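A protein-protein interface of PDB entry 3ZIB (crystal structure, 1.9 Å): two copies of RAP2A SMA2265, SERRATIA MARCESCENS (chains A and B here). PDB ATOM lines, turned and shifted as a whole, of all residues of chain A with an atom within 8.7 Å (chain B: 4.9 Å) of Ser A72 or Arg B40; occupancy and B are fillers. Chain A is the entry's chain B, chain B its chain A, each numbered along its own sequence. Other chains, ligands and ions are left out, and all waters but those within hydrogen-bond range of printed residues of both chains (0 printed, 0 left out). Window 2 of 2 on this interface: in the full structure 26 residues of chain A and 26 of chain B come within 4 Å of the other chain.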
ATOM      1  N   TYR A  68      -9.252  14.546   9.595  1.00  0.00           N
ATOM      2  CA  TYR A  68      -9.198  14.926  11.025  1.00  0.00           C
ATOM      3  C   TYR A  68     -10.130  14.006  11.769  1.00  0.00           C
ATOM      4  O   TYR A  68     -11.216  13.719  11.268  1.00  0.00           O
ATOM      5  CB  TYR A  68      -9.644  16.398  11.216  1.00  0.00           C
ATOM      6  CG  TYR A  68      -8.524  17.402  11.151  1.00  0.00           C
ATOM      7  CD1 TYR A  68      -7.457  17.228  10.243  1.00  0.00           C
ATOM      8  CD2 TYR A  68      -8.488  18.501  12.010  1.00  0.00           C
ATOM      9  CE1 TYR A  68      -6.417  18.120  10.167  1.00  0.00           C
ATOM     10  CE2 TYR A  68      -7.430  19.421  11.951  1.00  0.00           C
ATOM     11  CZ  TYR A  68      -6.389  19.212  11.022  1.00  0.00           C
ATOM     12  OH  TYR A  68      -5.322  20.099  10.913  1.00  0.00           O
ATOM     13  N   ASP A  69      -9.736  13.545  12.965  1.00  0.00           N
ATOM     14  CA  ASP A  69     -10.637  12.707  13.772  1.00  0.00           C
ATOM     15  C   ASP A  69     -11.708  13.603  14.353  1.00  0.00           C
ATOM     16  O   ASP A  69     -11.455  14.799  14.597  1.00  0.00           O
ATOM     17  CB  ASP A  69      -9.915  12.018  14.936  1.00  0.00           C
ATOM     18  CG  ASP A  69      -8.688  11.223  14.499  1.00  0.00           C
ATOM     19  OD1 ASP A  69      -8.819  10.335  13.623  1.00  0.00           O
ATOM     20  OD2 ASP A  69      -7.599  11.474  15.068  1.00  0.00           O
ATOM     21  N   SER A  70     -12.904  13.052  14.553  1.00  0.00           N
ATOM     22  CA  SER A  70     -13.931  13.788  15.270  1.00  0.00           C
ATOM     23  C   SER A  70     -14.978  12.884  15.878  1.00  0.00           C
ATOM     24  O   SER A  70     -15.650  12.108  15.173  1.00  0.00           O
ATOM     25  CB  SER A  70     -14.589  14.858  14.398  1.00  0.00           C
ATOM     26  OG  SER A  70     -15.797  14.402  13.829  1.00  0.00           O
ATOM     27  N   MET A  71     -15.101  13.014  17.196  1.00  0.00           N
ATOM     28  CA  MET A  71     -16.170  12.404  17.956  1.00  0.00           C
ATOM     29  C   MET A  71     -17.574  12.837  17.484  1.00  0.00           C
ATOM     30  O   MET A  71     -18.534  12.080  17.638  1.00  0.00           O
ATOM     31  CB  MET A  71     -15.969  12.667  19.461  1.00  0.00           C
ATOM     32  CG  MET A  71     -15.665  11.405  20.258  1.00  0.00           C
ATOM     33  SD  MET A  71     -16.681   9.994  19.719  1.00  0.00           S
ATOM     34  CE  MET A  71     -18.348  10.418  20.254  1.00  0.00           C
ATOM     35  N   SER A  72     -17.680  14.039  16.899  1.00  0.00           N
ATOM     36  CA  SER A  72     -18.961  14.563  16.389  1.00  0.00           C
ATOM     37  C   SER A  72     -19.327  13.971  15.014  1.00  0.00           C
ATOM     38  O   SER A  72     -20.472  14.045  14.596  1.00  0.00           O
ATOM     39  CB  SER A  72     -18.900  16.098  16.295  1.00  0.00           C
ATOM     40  OG  SER A  72     -17.821  16.496  15.463  1.00  0.00           O
ATOM     41  N   GLY A  73     -18.360  13.389  14.301  1.00  0.00           N
ATOM     42  CA  GLY A  73     -18.593  12.972  12.898  1.00  0.00           C
ATOM     43  C   GLY A  73     -18.707  14.124  11.904  1.00  0.00           C
ATOM     44  O   GLY A  73     -19.232  13.965  10.804  1.00  0.00           O
ATOM     45  N   GLU A  74     -18.269  15.318  12.294  1.00  0.00           N
ATOM     46  CA  GLU A  74     -18.220  16.462  11.363  1.00  0.00           C
ATOM     47  C   GLU A  74     -16.850  16.406  10.709  1.00  0.00           C
ATOM     48  O   GLU A  74     -15.945  15.865  11.313  1.00  0.00           O
ATOM     49  CB  GLU A  74     -18.322  17.782  12.136  1.00  0.00           C
ATOM     50  CG  GLU A  74     -19.670  18.099  12.724  1.00  0.00           C
ATOM     51  CD  GLU A  74     -20.729  18.210  11.663  1.00  0.00           C
ATOM     52  OE1 GLU A  74     -20.411  18.638  10.521  1.00  0.00           O
ATOM     53  OE2 GLU A  74     -21.882  17.861  11.975  1.00  0.00           O
ATOM     54  N   PRO A  75     -16.679  17.000   9.506  1.00  0.00           N
ATOM     55  CA  PRO A  75     -15.355  16.896   8.881  1.00  0.00           C
ATOM     56  C   PRO A  75     -14.243  17.707   9.575  1.00  0.00           C
ATOM     57  O   PRO A  75     -13.065  17.416   9.373  1.00  0.00           O
ATOM     58  CB  PRO A  75     -15.598  17.454   7.488  1.00  0.00           C
ATOM     59  CG  PRO A  75     -16.780  18.353   7.622  1.00  0.00           C
ATOM     60  CD  PRO A  75     -17.640  17.720   8.645  1.00  0.00           C
ATOM     61  N   MET A  76     -14.602  18.695  10.397  1.00  0.00           N
ATOM     62  CA  MET A  76     -13.604  19.563  11.131  1.00  0.00           C
ATOM     63  C   MET A  76     -12.871  20.521  10.190  1.00  0.00           C
ATOM     64  O   MET A  76     -11.688  20.846  10.362  1.00  0.00           O
ATOM     65  CB  MET A  76     -12.627  18.739  11.962  1.00  0.00           C
ATOM     66  CG  MET A  76     -13.269  17.658  12.806  1.00  0.00           C
ATOM     67  SD  MET A  76     -14.474  18.265  14.032  1.00  0.00           S
ATOM     68  CE  MET A  76     -15.420  19.529  13.188  1.00  0.00           C
ATOM     69  N   ALA B  36     -19.418  24.728  15.199  1.00  0.00           N
ATOM     70  CA  ALA B  36     -19.814  24.326  16.588  1.00  0.00           C
ATOM     71  C   ALA B  36     -18.995  23.153  17.161  1.00  0.00           C
ATOM     72  O   ALA B  36     -18.635  23.174  18.352  1.00  0.00           O
ATOM     73  CB  ALA B  36     -21.288  24.025  16.679  1.00  0.00           C
ATOM     74  N   ALA B  37     -18.709  22.133  16.346  1.00  0.00           N
ATOM     75  CA  ALA B  37     -17.936  20.999  16.853  1.00  0.00           C
ATOM     76  C   ALA B  37     -16.484  21.424  17.132  1.00  0.00           C
ATOM     77  O   ALA B  37     -15.886  21.038  18.137  1.00  0.00           O
ATOM     78  CB  ALA B  37     -17.985  19.809  15.923  1.00  0.00           C
ATOM     79  N   ALA B  38     -15.941  22.264  16.287  1.00  0.00           N
ATOM     80  CA  ALA B  38     -14.623  22.848  16.511  1.00  0.00           C
ATOM     81  C   ALA B  38     -14.678  23.664  17.816  1.00  0.00           C
ATOM     82  O   ALA B  38     -13.786  23.542  18.622  1.00  0.00           O
ATOM     83  CB  ALA B  38     -14.215  23.761  15.321  1.00  0.00           C
ATOM     84  N   ALA B  39     -15.687  24.511  17.990  1.00  0.00           N
ATOM     85  CA  ALA B  39     -15.744  25.348  19.208  1.00  0.00           C
ATOM     86  C   ALA B  39     -15.777  24.443  20.450  1.00  0.00           C
ATOM     87  O   ALA B  39     -15.092  24.720  21.456  1.00  0.00           O
ATOM     88  CB  ALA B  39     -16.992  26.234  19.198  1.00  0.00           C
ATOM     89  N   ARG B  40     -16.536  23.350  20.384  1.00  0.00           N
ATOM     90  CA  ARG B  40     -16.601  22.453  21.548  1.00  0.00           C
ATOM     91  C   ARG B  40     -15.226  21.897  21.805  1.00  0.00           C
ATOM     92  O   ARG B  40     -14.795  21.788  22.947  1.00  0.00           O
ATOM     93  CB  ARG B  40     -17.615  21.306  21.341  1.00  0.00           C
ATOM     94  CG  ARG B  40     -19.058  21.798  21.406  1.00  0.00           C
ATOM     95  CD  ARG B  40     -20.066  20.641  21.537  1.00  0.00           C
ATOM     96  NE  ARG B  40     -19.954  19.679  20.425  1.00  0.00           N
ATOM     97  CZ  ARG B  40     -20.524  19.805  19.206  1.00  0.00           C
ATOM     98  NH1 ARG B  40     -21.262  20.857  18.885  1.00  0.00           N
ATOM     99  NH2 ARG B  40     -20.351  18.860  18.291  1.00  0.00           N
ATOM    100  N   GLY B  41     -14.509  21.528  20.760  1.00  0.00           N
ATOM    101  CA  GLY B  41     -13.142  21.014  20.952  1.00  0.00           C
ATOM    102  C   GLY B  41     -12.140  22.005  21.579  1.00  0.00           C
ATOM    103  O   GLY B  41     -11.270  21.617  22.387  1.00  0.00           O
ATOM    104  N   TYR B  42     -12.205  23.286  21.182  1.00  0.00           N
ATOM    105  CA  TYR B  42     -11.362  24.327  21.781  1.00  0.00           C
ATOM    106  C   TYR B  42     -11.755  24.599  23.221  1.00  0.00           C
ATOM    107  O   TYR B  42     -10.913  24.979  24.020  1.00  0.00           O
ATOM    108  CB  TYR B  42     -11.432  25.610  20.909  1.00  0.00           C
ATOM    109  CG  TYR B  42     -10.853  25.339  19.514  1.00  0.00           C
ATOM    110  CD1 TYR B  42      -9.616  24.682  19.337  1.00  0.00           C
ATOM    111  CD2 TYR B  42     -11.564  25.737  18.384  1.00  0.00           C
ATOM    112  CE1 TYR B  42      -9.086  24.428  18.046  1.00  0.00           C
ATOM    113  CE2 TYR B  42     -11.052  25.512  17.123  1.00  0.00           C
ATOM    114  CZ  TYR B  42      -9.862  24.845  16.949  1.00  0.00           C
ATOM    115  OH  TYR B  42      -9.484  24.681  15.643  1.00  0.00           O
ATOM    116  N   THR B  43     -13.030  24.383  23.573  1.00  0.00           N
ATOM    117  CA  THR B  43     -13.412  24.554  24.965  1.00  0.00           C
ATOM    118  C   THR B  43     -12.846  23.410  25.781  1.00  0.00           C
ATOM    119  O   THR B  43     -12.220  23.668  26.800  1.00  0.00           O
ATOM    120  CB  THR B  43     -14.929  24.593  25.196  1.00  0.00           C
ATOM    121  OG1 THR B  43     -15.522  25.550  24.320  1.00  0.00           O
ATOM    122  CG2 THR B  43     -15.249  25.049  26.672  1.00  0.00           C
ATOM    123  N   GLU B  44     -13.029  22.169  25.324  1.00  0.00           N
ATOM    124  CA  GLU B  44     -12.510  20.994  26.068  1.00  0.00           C
ATOM    125  C   GLU B  44     -10.980  20.925  26.208  1.00  0.00           C
ATOM    126  O   GLU B  44     -10.459  20.555  27.254  1.00  0.00           O
ATOM    127  CB  GLU B  44     -13.063  19.694  25.477  1.00  0.00           C
ATOM    128  CG  GLU B  44     -12.205  18.459  25.699  1.00  0.00           C
ATOM    129  CD  GLU B  44     -12.798  17.263  24.998  1.00  0.00           C
ATOM    130  OE1 GLU B  44     -14.030  17.285  24.770  1.00  0.00           O
ATOM    131  OE2 GLU B  44     -12.041  16.338  24.665  1.00  0.00           O
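The side-chain hydroxyl (OG) of Ser A72 lies close to the backbone NH (N) of Glu A74, at 3.4 Å.
The side-chain hydroxyl (OG) of Ser A70 sits at hydrogen-bond distance from the backbone carbonyl oxygen (O) of Glu A74, at 2.9 Å.
The side-chain hydroxyl (OG) of Ser A70 is in hydrogen-bond range of the side-chain hydroxyl (OG) of Ser A72 (3.3 Å).
Among the printed residues, pairs that only touch across the chains: Ser A72 with Ala B37, Ser A72 with Arg B40, Met A76 with Ala B37 and Glu A74 with Ala B37.
Ser A72 touches just these residues of chain B: Ala B37 and Arg B40.
No residue of chain A comes within 4 Å of Gly B41.
Of the printed residues of chain A, Ala B37 touches Ser A72, Glu A74 and Met A76.
Printed residues of chain B within 4 Å of Glu A74: Ala B37.
Of the printed residues of chain B, Met A76 touches Ala B37 (3.8 Å).
The nearest residue of chain A that does not touch Arg B40 is Glu A74 (5.7 Å).
Hydrophobic or aromatic side chains of chain B that line the printed part of chain A: Ala B37.
Printed residues of chain A that touch a printed residue of chain B: Ser A72, Glu A74 and Met A76.
Among the printed residues, 4 pairs touch across the chains.
Among the printed residues, no Asp or Glu carboxylate lies within 4 Å of a Lys or Arg side-chain nitrogen of the other chain.
No position is printed for both chains.
Of the 4 pairs that touch across the chains among the printed residues, none has its exchanged pair printed and touching as well.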
